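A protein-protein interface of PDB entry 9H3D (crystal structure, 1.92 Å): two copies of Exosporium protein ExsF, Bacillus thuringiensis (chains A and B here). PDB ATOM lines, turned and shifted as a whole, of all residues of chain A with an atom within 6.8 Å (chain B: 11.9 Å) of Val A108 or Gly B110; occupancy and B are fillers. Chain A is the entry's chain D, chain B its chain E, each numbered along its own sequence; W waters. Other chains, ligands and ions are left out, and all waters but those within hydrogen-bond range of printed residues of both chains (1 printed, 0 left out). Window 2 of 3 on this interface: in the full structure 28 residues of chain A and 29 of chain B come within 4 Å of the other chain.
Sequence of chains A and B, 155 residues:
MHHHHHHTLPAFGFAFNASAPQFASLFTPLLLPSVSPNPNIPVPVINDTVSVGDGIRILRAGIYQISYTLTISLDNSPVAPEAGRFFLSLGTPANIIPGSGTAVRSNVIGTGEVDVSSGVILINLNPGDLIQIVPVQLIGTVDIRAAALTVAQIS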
ATOM      1  N   LEU A  74      11.262  27.454  22.466  1.00  0.00           N
ATOM      2  CA  LEU A  74      11.859  27.223  21.156  1.00  0.00           C
ATOM      3  C   LEU A  74      11.689  25.772  20.709  1.00  0.00           C
ATOM      4  O   LEU A  74      12.609  25.169  20.151  1.00  0.00           O
ATOM      5  CB  LEU A  74      13.337  27.604  21.168  1.00  0.00           C
ATOM      6  CG  LEU A  74      13.565  29.066  21.590  1.00  0.00           C
ATOM      7  CD1 LEU A  74      15.031  29.302  21.886  1.00  0.00           C
ATOM      8  CD2 LEU A  74      13.059  29.990  20.511  1.00  0.00           C
ATOM      9  N   ASP A  75      10.501  25.206  20.910  1.00  0.00           N
ATOM     10  CA  ASP A  75      10.228  23.797  20.621  1.00  0.00           C
ATOM     11  C   ASP A  75       9.049  23.635  19.664  1.00  0.00           C
ATOM     12  O   ASP A  75       8.251  22.704  19.782  1.00  0.00           O
ATOM     13  CB  ASP A  75       9.979  23.029  21.917  1.00  0.00           C
ATOM     14  CG  ASP A  75       8.858  23.638  22.751  1.00  0.00           C
ATOM     15  OD1 ASP A  75       8.316  24.673  22.336  1.00  0.00           O
ATOM     16  OD2 ASP A  75       8.506  23.079  23.812  1.00  0.00           O
ATOM     17  N   ALA A  80      13.324  22.906  11.982  1.00  0.00           N
ATOM     18  CA  ALA A  80      14.040  24.177  11.963  1.00  0.00           C
ATOM     19  C   ALA A  80      14.345  24.644  13.378  1.00  0.00           C
ATOM     20  O   ALA A  80      13.418  25.023  14.115  1.00  0.00           O
ATOM     21  CB  ALA A  80      13.225  25.240  11.222  1.00  0.00           C
ATOM     22  N   PRO A  81      15.610  24.641  13.794  1.00  0.00           N
ATOM     23  CA  PRO A  81      15.975  25.278  15.068  1.00  0.00           C
ATOM     24  C   PRO A  81      15.629  26.762  15.054  1.00  0.00           C
ATOM     25  O   PRO A  81      15.710  27.421  14.023  1.00  0.00           O
ATOM     26  CB  PRO A  81      17.483  25.033  15.152  1.00  0.00           C
ATOM     27  CG  PRO A  81      17.646  23.691  14.398  1.00  0.00           C
ATOM     28  CD  PRO A  81      16.722  23.864  13.218  1.00  0.00           C
ATOM     29  N   GLU A  82      15.202  27.273  16.204  1.00  0.00           N
ATOM     30  CA  GLU A  82      14.477  28.533  16.279  1.00  0.00           C
ATOM     31  C   GLU A  82      15.287  29.621  16.991  1.00  0.00           C
ATOM     32  O   GLU A  82      16.180  29.334  17.793  1.00  0.00           O
ATOM     33  CB  GLU A  82      13.127  28.309  16.962  1.00  0.00           C
ATOM     34  CG  GLU A  82      12.159  27.619  16.009  1.00  0.00           C
ATOM     35  CD  GLU A  82      11.027  26.869  16.696  1.00  0.00           C
ATOM     36  OE1 GLU A  82      10.986  26.828  17.939  1.00  0.00           O
ATOM     37  OE2 GLU A  82      10.152  26.338  15.972  1.00  0.00           O
ATOM     38  N   ARG A 105      18.948  32.092  20.562  1.00  0.00           N
ATOM     39  CA  ARG A 105      19.008  31.200  19.406  1.00  0.00           C
ATOM     40  C   ARG A 105      19.388  29.787  19.826  1.00  0.00           C
ATOM     41  O   ARG A 105      20.374  29.585  20.543  1.00  0.00           O
ATOM     42  CB  ARG A 105      20.013  31.697  18.364  1.00  0.00           C
ATOM     43  CG  ARG A 105      20.342  30.637  17.301  1.00  0.00           C
ATOM     44  CD  ARG A 105      21.180  31.202  16.166  1.00  0.00           C
ATOM     45  NE  ARG A 105      22.439  31.769  16.638  1.00  0.00           N
ATOM     46  CZ  ARG A 105      23.597  31.122  16.621  1.00  0.00           C
ATOM     47  NH1 ARG A 105      23.700  29.897  16.121  1.00  0.00           N
ATOM     48  NH2 ARG A 105      24.675  31.709  17.135  1.00  0.00           N
ATOM     49  N   SER A 106      18.627  28.811  19.345  1.00  0.00           N
ATOM     50  CA  SER A 106      18.929  27.410  19.580  1.00  0.00           C
ATOM     51  C   SER A 106      19.270  26.731  18.261  1.00  0.00           C
ATOM     52  O   SER A 106      18.584  26.938  17.255  1.00  0.00           O
ATOM     53  CB  SER A 106      17.750  26.697  20.232  1.00  0.00           C
ATOM     54  OG  SER A 106      18.017  25.317  20.271  1.00  0.00           O
ATOM     55  N   ASN A 107      20.324  25.921  18.268  1.00  0.00           N
ATOM     56  CA  ASN A 107      20.737  25.195  17.078  1.00  0.00           C
ATOM     57  C   ASN A 107      20.096  23.819  16.979  1.00  0.00           C
ATOM     58  O   ASN A 107      20.411  23.074  16.045  1.00  0.00           O
ATOM     59  CB  ASN A 107      22.257  25.051  17.044  1.00  0.00           C
ATOM     60  CG  ASN A 107      22.965  26.393  17.069  1.00  0.00           C
ATOM     61  OD1 ASN A 107      22.510  27.363  16.446  1.00  0.00           O
ATOM     62  ND2 ASN A 107      24.075  26.461  17.796  1.00  0.00           N
ATOM     63  N   VAL A 108      19.196  23.472  17.900  1.00  0.00           N
ATOM     64  CA  VAL A 108      18.541  22.174  17.890  1.00  0.00           C
ATOM     65  C   VAL A 108      17.043  22.374  18.069  1.00  0.00           C
ATOM     66  O   VAL A 108      16.586  23.373  18.630  1.00  0.00           O
ATOM     67  CB  VAL A 108      19.090  21.230  18.980  1.00  0.00           C
ATOM     68  CG1 VAL A 108      20.561  20.914  18.728  1.00  0.00           C
ATOM     69  CG2 VAL A 108      18.882  21.818  20.349  1.00  0.00           C
ATOM     70  N   ILE A 109      16.274  21.396  17.583  1.00  0.00           N
ATOM     71  CA  ILE A 109      14.834  21.437  17.787  1.00  0.00           C
ATOM     72  C   ILE A 109      14.515  20.998  19.212  1.00  0.00           C
ATOM     73  O   ILE A 109      15.320  20.348  19.886  1.00  0.00           O
ATOM     74  CB  ILE A 109      14.095  20.571  16.749  1.00  0.00           C
ATOM     75  CG1 ILE A 109      14.440  19.090  16.926  1.00  0.00           C
ATOM     76  CG2 ILE A 109      14.425  21.029  15.333  1.00  0.00           C
ATOM     77  CD1 ILE A 109      13.481  18.158  16.179  1.00  0.00           C
ATOM     78  N   GLY A 110      13.337  21.393  19.691  1.00  0.00           N
ATOM     79  CA  GLY A 110      12.870  20.899  20.979  1.00  0.00           C
ATOM     80  C   GLY A 110      13.473  21.551  22.204  1.00  0.00           C
ATOM     81  O   GLY A 110      13.618  20.896  23.243  1.00  0.00           O
ATOM     82  N   THR A 111      13.814  22.832  22.121  1.00  0.00           N
ATOM     83  CA  THR A 111      14.368  23.568  23.245  1.00  0.00           C
ATOM     84  C   THR A 111      13.241  24.195  24.054  1.00  0.00           C
ATOM     85  O   THR A 111      12.403  24.911  23.505  1.00  0.00           O
ATOM     86  CB  THR A 111      15.322  24.645  22.725  1.00  0.00           C
ATOM     87  OG1 THR A 111      16.406  24.004  22.037  1.00  0.00           O
ATOM     88  CG2 THR A 111      15.868  25.509  23.872  1.00  0.00           C
ATOM     89  N   ILE B  72      24.994  36.754  24.703  1.00  0.00           N
ATOM     90  CA  ILE B  72      26.178  35.907  24.675  1.00  0.00           C
ATOM     91  C   ILE B  72      25.958  34.762  23.702  1.00  0.00           C
ATOM     92  O   ILE B  72      25.048  33.940  23.892  1.00  0.00           O
ATOM     93  CB  ILE B  72      26.508  35.349  26.065  1.00  0.00           C
ATOM     94  CG1 ILE B  72      26.632  36.481  27.083  1.00  0.00           C
ATOM     95  CG2 ILE B  72      27.784  34.569  25.992  1.00  0.00           C
ATOM     96  CD1 ILE B  72      26.855  35.967  28.507  1.00  0.00           C
ATOM     97  N   SER B  73      26.827  34.660  22.702  1.00  0.00           N
ATOM     98  CA  SER B  73      26.821  33.494  21.828  1.00  0.00           C
ATOM     99  C   SER B  73      27.717  32.405  22.409  1.00  0.00           C
ATOM    100  O   SER B  73      28.897  32.651  22.687  1.00  0.00           O
ATOM    101  CB  SER B  73      27.297  33.852  20.423  1.00  0.00           C
ATOM    102  OG  SER B  73      27.431  32.660  19.658  1.00  0.00           O
ATOM    103  N   LEU B  74      27.159  31.199  22.572  1.00  0.00           N
ATOM    104  CA  LEU B  74      27.901  30.049  23.078  1.00  0.00           C
ATOM    105  C   LEU B  74      28.232  29.050  21.986  1.00  0.00           C
ATOM    106  O   LEU B  74      28.493  27.885  22.284  1.00  0.00           O
ATOM    107  CB  LEU B  74      27.123  29.351  24.192  1.00  0.00           C
ATOM    108  CG  LEU B  74      26.788  30.323  25.315  1.00  0.00           C
ATOM    109  CD1 LEU B  74      25.939  29.673  26.386  1.00  0.00           C
ATOM    110  CD2 LEU B  74      28.099  30.948  25.888  1.00  0.00           C
ATOM    111  N   ASP B  75      28.215  29.468  20.719  1.00  0.00           N
ATOM    112  CA  ASP B  75      28.597  28.545  19.653  1.00  0.00           C
ATOM    113  C   ASP B  75      29.602  29.188  18.706  1.00  0.00           C
ATOM    114  O   ASP B  75      29.675  28.830  17.529  1.00  0.00           O
ATOM    115  CB  ASP B  75      27.368  28.013  18.902  1.00  0.00           C
ATOM    116  CG  ASP B  75      26.766  29.016  17.915  1.00  0.00           C
ATOM    117  OD1 ASP B  75      26.893  30.242  18.112  1.00  0.00           O
ATOM    118  OD2 ASP B  75      26.135  28.559  16.934  1.00  0.00           O
ATOM    119  N   ASN B  76      30.391  30.131  19.209  1.00  0.00           N
ATOM    120  CA  ASN B  76      31.470  30.717  18.419  1.00  0.00           C
ATOM    121  C   ASN B  76      32.821  30.284  18.995  1.00  0.00           C
ATOM    122  O   ASN B  76      33.730  31.103  19.168  1.00  0.00           O
ATOM    123  CB  ASN B  76      31.329  32.247  18.399  1.00  0.00           C
ATOM    124  CG  ASN B  76      31.993  32.881  17.192  1.00  0.00           C
ATOM    125  OD1 ASN B  76      32.695  32.210  16.430  1.00  0.00           O
ATOM    126  ND2 ASN B  76      31.778  34.184  17.012  1.00  0.00           N
ATOM    127  N   SER B  77      32.955  28.993  19.297  1.00  0.00           N
ATOM    128  CA  SER B  77      34.038  28.470  20.114  1.00  0.00           C
ATOM    129  C   SER B  77      34.573  27.181  19.515  1.00  0.00           C
ATOM    130  O   SER B  77      33.789  26.331  19.059  1.00  0.00           O
ATOM    131  CB  SER B  77      33.580  28.191  21.552  1.00  0.00           C
ATOM    132  OG  SER B  77      34.628  27.630  22.336  1.00  0.00           O
ATOM    133  N   PRO B  78      35.897  27.001  19.513  1.00  0.00           N
ATOM    134  CA  PRO B  78      36.473  25.756  18.993  1.00  0.00           C
ATOM    135  C   PRO B  78      36.360  24.582  19.955  1.00  0.00           C
ATOM    136  O   PRO B  78      36.611  23.438  19.542  1.00  0.00           O
ATOM    137  CB  PRO B  78      37.940  26.135  18.755  1.00  0.00           C
ATOM    138  CG  PRO B  78      38.210  27.194  19.794  1.00  0.00           C
ATOM    139  CD  PRO B  78      36.931  27.976  19.911  1.00  0.00           C
ATOM    140  N   VAL B  79      36.010  24.820  21.222  1.00  0.00           N
ATOM    141  CA  VAL B  79      35.827  23.746  22.188  1.00  0.00           C
ATOM    142  C   VAL B  79      34.525  23.983  22.938  1.00  0.00           C
ATOM    143  O   VAL B  79      34.000  25.100  22.990  1.00  0.00           O
ATOM    144  CB  VAL B  79      37.000  23.623  23.194  1.00  0.00           C
ATOM    145  CG1 VAL B  79      38.346  23.449  22.474  1.00  0.00           C
ATOM    146  CG2 VAL B  79      37.024  24.814  24.136  1.00  0.00           C
ATOM    147  N   ALA B  80      33.996  22.902  23.504  1.00  0.00           N
ATOM    148  CA  ALA B  80      32.922  22.938  24.478  1.00  0.00           C
ATOM    149  C   ALA B  80      33.433  22.345  25.786  1.00  0.00           C
ATOM    150  O   ALA B  80      34.352  21.516  25.776  1.00  0.00           O
ATOM    151  CB  ALA B  80      31.689  22.161  23.996  1.00  0.00           C
ATOM    152  N   PRO B  81      32.883  22.750  26.930  1.00  0.00           N
ATOM    153  CA  PRO B  81      31.795  23.715  27.143  1.00  0.00           C
ATOM    154  C   PRO B  81      32.148  25.158  26.769  1.00  0.00           C
ATOM    155  O   PRO B  81      33.304  25.521  26.548  1.00  0.00           O
ATOM    156  CB  PRO B  81      31.524  23.607  28.654  1.00  0.00           C
ATOM    157  CG  PRO B  81      32.251  22.392  29.132  1.00  0.00           C
ATOM    158  CD  PRO B  81      33.394  22.212  28.199  1.00  0.00           C
ATOM    159  N   GLU B  82      31.103  25.973  26.672  1.00  0.00           N
ATOM    160  CA  GLU B  82      31.192  27.419  26.567  1.00  0.00           C
ATOM    161  C   GLU B  82      30.474  27.987  27.777  1.00  0.00           C
ATOM    162  O   GLU B  82      29.289  27.695  27.983  1.00  0.00           O
ATOM    163  CB  GLU B  82      30.552  27.924  25.271  1.00  0.00           C
ATOM    164  CG  GLU B  82      31.144  27.297  24.027  1.00  0.00           C
ATOM    165  CD  GLU B  82      30.378  26.073  23.560  1.00  0.00           C
ATOM    166  OE1 GLU B  82      29.387  25.705  24.217  1.00  0.00           O
ATOM    167  OE2 GLU B  82      30.756  25.498  22.519  1.00  0.00           O
ATOM    168  N   ALA B  83      31.191  28.772  28.581  1.00  0.00           N
ATOM    169  CA  ALA B  83      30.692  29.197  29.882  1.00  0.00           C
ATOM    170  C   ALA B  83      31.375  30.495  30.296  1.00  0.00           C
ATOM    171  O   ALA B  83      32.527  30.747  29.938  1.00  0.00           O
ATOM    172  CB  ALA B  83      30.950  28.126  30.941  1.00  0.00           C
ATOM    173  N   ARG B 105      26.421  28.566  31.012  1.00  0.00           N
ATOM    174  CA  ARG B 105      27.299  27.473  30.627  1.00  0.00           C
ATOM    175  C   ARG B 105      26.529  26.524  29.723  1.00  0.00           C
ATOM    176  O   ARG B 105      25.455  26.048  30.092  1.00  0.00           O
ATOM    177  CB  ARG B 105      27.817  26.738  31.869  1.00  0.00           C
ATOM    178  CG  ARG B 105      28.545  25.438  31.591  1.00  0.00           C
ATOM    179  CD  ARG B 105      29.279  24.966  32.824  1.00  0.00           C
ATOM    180  NE  ARG B 105      28.387  24.722  33.947  1.00  0.00           N
ATOM    181  CZ  ARG B 105      27.940  23.522  34.298  1.00  0.00           C
ATOM    182  NH1 ARG B 105      28.244  22.440  33.601  1.00  0.00           N
ATOM    183  NH2 ARG B 105      27.168  23.406  35.374  1.00  0.00           N
ATOM    184  N   SER B 106      27.079  26.254  28.549  1.00  0.00           N
ATOM    185  CA  SER B 106      26.551  25.242  27.650  1.00  0.00           C
ATOM    186  C   SER B 106      27.587  24.137  27.546  1.00  0.00           C
ATOM    187  O   SER B 106      28.731  24.390  27.146  1.00  0.00           O
ATOM    188  CB  SER B 106      26.228  25.822  26.276  1.00  0.00           C
ATOM    189  OG  SER B 106      25.854  24.793  25.380  1.00  0.00           O
ATOM    190  N   ASN B 107      27.184  22.916  27.903  1.00  0.00           N
ATOM    191  CA  ASN B 107      28.095  21.786  27.888  1.00  0.00           C
ATOM    192  C   ASN B 107      28.284  21.187  26.505  1.00  0.00           C
ATOM    193  O   ASN B 107      29.192  20.369  26.327  1.00  0.00           O
ATOM    194  CB  ASN B 107      27.599  20.717  28.856  1.00  0.00           C
ATOM    195  CG  ASN B 107      27.535  21.227  30.277  1.00  0.00           C
ATOM    196  OD1 ASN B 107      28.374  22.019  30.694  1.00  0.00           O
ATOM    197  ND2 ASN B 107      26.528  20.789  31.024  1.00  0.00           N
ATOM    198  N   VAL B 108      27.456  21.564  25.533  1.00  0.00           N
ATOM    199  CA  VAL B 108      27.556  21.037  24.178  1.00  0.00           C
ATOM    200  C   VAL B 108      27.527  22.189  23.179  1.00  0.00           C
ATOM    201  O   VAL B 108      27.885  23.328  23.508  1.00  0.00           O
ATOM    202  CB  VAL B 108      26.430  20.022  23.900  1.00  0.00           C
ATOM    203  CG1 VAL B 108      26.456  18.903  24.932  1.00  0.00           C
ATOM    204  CG2 VAL B 108      25.077  20.709  23.906  1.00  0.00           C
ATOM    205  N   ILE B 109      27.107  21.905  21.946  1.00  0.00           N
ATOM    206  CA  ILE B 109      27.206  22.872  20.865  1.00  0.00           C
ATOM    207  C   ILE B 109      25.838  23.249  20.301  1.00  0.00           C
ATOM    208  O   ILE B 109      25.755  23.947  19.286  1.00  0.00           O
ATOM    209  CB  ILE B 109      28.152  22.354  19.760  1.00  0.00           C
ATOM    210  CG1 ILE B 109      28.662  23.511  18.885  1.00  0.00           C
ATOM    211  CG2 ILE B 109      27.478  21.230  18.950  1.00  0.00           C
ATOM    212  CD1 ILE B 109      29.134  24.736  19.680  1.00  0.00           C
ATOM    213  N   GLY B 110      24.760  22.843  20.961  1.00  0.00           N
ATOM    214  CA  GLY B 110      23.443  23.145  20.445  1.00  0.00           C
ATOM    215  C   GLY B 110      22.878  24.504  20.784  1.00  0.00           C
ATOM    216  O   GLY B 110      21.683  24.732  20.566  1.00  0.00           O
ATOM    217  N   THR B 111      23.688  25.433  21.294  1.00  0.00           N
ATOM    218  CA  THR B 111      23.173  26.709  21.777  1.00  0.00           C
ATOM    219  C   THR B 111      23.921  27.862  21.126  1.00  0.00           C
ATOM    220  O   THR B 111      25.153  27.930  21.203  1.00  0.00           O
ATOM    221  CB  THR B 111      23.285  26.813  23.298  1.00  0.00           C
ATOM    222  OG1 THR B 111      22.557  25.741  23.910  1.00  0.00           O
ATOM    223  CG2 THR B 111      22.710  28.125  23.764  1.00  0.00           C
ATOM    224  N   GLY B 112      23.172  28.770  20.499  1.00  0.00           N
ATOM    225  CA  GLY B 112      23.740  30.015  20.026  1.00  0.00           C
ATOM    226  C   GLY B 112      23.655  31.086  21.095  1.00  0.00           C
ATOM    227  O   GLY B 112      24.235  30.930  22.181  1.00  0.00           O
ATOM    228  N   GLU B 113      22.907  32.156  20.816  1.00  0.00           N
ATOM    229  CA  GLU B 113      22.796  33.262  21.752  1.00  0.00           C
ATOM    230  C   GLU B 113      21.914  32.899  22.942  1.00  0.00           C
ATOM    231  O   GLU B 113      20.894  32.213  22.802  1.00  0.00           O
ATOM    232  CB  GLU B 113      22.228  34.509  21.064  1.00  0.00           C
ATOM    233  CG  GLU B 113      23.244  35.286  20.254  1.00  0.00           C
ATOM    234  CD  GLU B 113      23.555  34.596  18.945  1.00  0.00           C
ATOM    235  OE1 GLU B 113      22.654  33.932  18.400  1.00  0.00           O
ATOM    236  OE2 GLU B 113      24.695  34.714  18.454  1.00  0.00           O
ATOM    237  N   VAL B 114      22.325  33.372  24.122  1.00  0.00           N
ATOM    238  CA  VAL B 114      21.524  33.295  25.334  1.00  0.00           C
ATOM    239  C   VAL B 114      21.499  34.687  25.936  1.00  0.00           C
ATOM    240  O   VAL B 114      22.315  35.545  25.602  1.00  0.00           O
ATOM    241  CB  VAL B 114      22.065  32.271  26.362  1.00  0.00           C
ATOM    242  CG1 VAL B 114      22.305  30.953  25.701  1.00  0.00           C
ATOM    243  CG2 VAL B 114      23.342  32.783  27.023  1.00  0.00           C
ATOM    244  N   THR B 141      35.406  29.750  24.196  1.00  0.00           N
ATOM    245  CA  THR B 141      35.253  31.111  23.693  1.00  0.00           C
ATOM    246  C   THR B 141      33.836  31.591  23.958  1.00  0.00           C
ATOM    247  O   THR B 141      32.873  30.875  23.665  1.00  0.00           O
ATOM    248  CB  THR B 141      35.525  31.197  22.194  1.00  0.00           C
ATOM    249  OG1 THR B 141      36.850  30.733  21.905  1.00  0.00           O
ATOM    250  CG2 THR B 141      35.394  32.656  21.739  1.00  0.00           C
HETATM  251  O   HOH W   1      19.852  25.190  22.534  1.00  0.00           O
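The guanidinium group of Arg A105 lies within salt-bridge range of the side-chain carboxylate of Glu B113, 2.8 Å away. The side-chain carboxylate of Asp B75 lies within salt-bridge range of the guanidinium group of Arg A105 (2.8 Å). N of Gly B112 is in hydrogen-bond range of O of Arg A105 (2.9 Å). ND2 of Asn A107 lies within hydrogen-bond range of OD2 of Asp B75, 3.1 Å away. The backbone NH of Asn A107 sits at hydrogen-bond distance from the backbone carbonyl oxygen of Gly B110 (2.9 Å). The backbone carbonyl oxygen of Ile B109 lies within hydrogen-bond range of the side-chain amide nitrogen of Asn A107, 3.4 Å away.
O of Val A108 sits at hydrogen-bond distance from OG1 of Thr A111 (3.5 Å). O of Thr B111 lies close to N of Asp B75. OG of Ser A106 lies within hydrogen-bond range of OG1 of Thr A111 (2.7 Å). The guanidinium group of Arg A105 is in hydrogen-bond range of the side-chain amide oxygen of Asn A107, 2.8 Å away. The side-chain hydroxyl (OG) of Ser B73 sits at hydrogen-bond distance from the side-chain carboxylate (OD1) of Asp B75 (2.9 Å). The backbone NH of Leu B74 lies within hydrogen-bond range of the backbone carbonyl oxygen of Gly B112 (3.0 Å).
Among the printed residues, pairs that only touch across the chains: Arg A105 with Ser B73, Arg A105 with Thr B111, Ser A106 with Gly B110, Asn A107 with Thr B111, Asn A107 with Gly B112 and Val A108 with Gly B110.
Val A108 touches just one residue of chain B: Gly B110 (3.9 Å). No residue of chain B comes within 4 Å of Leu A74. Glu A82 touches none of the printed residues of chain B. Ser A106 touches just one residue of chain B: Gly B110 (3.7 Å). Asn A107 touches just these residues of chain B: Asp B75 (3.1 Å), Ile B109 (3.4 Å), Gly B110 (2.9 Å), Thr B111 (3.6 Å) and Gly B112 (3.7 Å). No residue of chain B comes within 4 Å of Ile A109. No residue of chain B comes within 4 Å of Gly A110. Thr A111 touches none of the printed residues of chain B. Printed residues of chain B within 4 Å of Arg A105: Ser B73, Asp B75, Thr B111, Gly B112 and Glu B113. Of the printed residues of chain A, Glu B113 touches Arg A105 (2.8 Å). Of the printed residues of chain A, Asp B75 touches Arg A105 (2.8 Å) and Asn A107 (3.1 Å). Ala B80 touches none of the printed residues of chain A.
Printed residues of chain A that touch a printed residue of chain B: Arg A105, Ser A106, Asn A107 and Val A108. Printed residues of chain B that touch a printed residue of chain A: Ser B73, Asp B75, Ile B109, Gly B110, Thr B111, Gly B112 and Glu B113. Along chain B the printed residues that touch a printed residue of chain A span positions 73 to 113. Among the printed residues, 12 pairs touch across the chains.
Arg A105 touches Thr B111, but with the chains exchanged Thr A111 does not touch Arg B105 (11.4 Å). Asn A107 touches Ile B109, but with the chains exchanged Ile A109 does not touch Asn B107 (14.5 Å). Asn A107 touches Gly B110, but with the chains exchanged Gly A110 does not touch Asn B107 (14.5 Å). Val A108 touches Gly B110, but with the chains exchanged Gly A110 does not touch Val B108 (11.5 Å). Of the 12 pairs that touch across the chains among the printed residues, none has its exchanged pair printed and touching as well.
Water W1 lies within hydrogen-bond range of the backbone carbonyl oxygen of Gly B110 (2.7 Å), the side-chain hydroxyl of Ser A106 (2.9 Å) and the side-chain hydroxyl of Thr B111 (3.1 Å).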
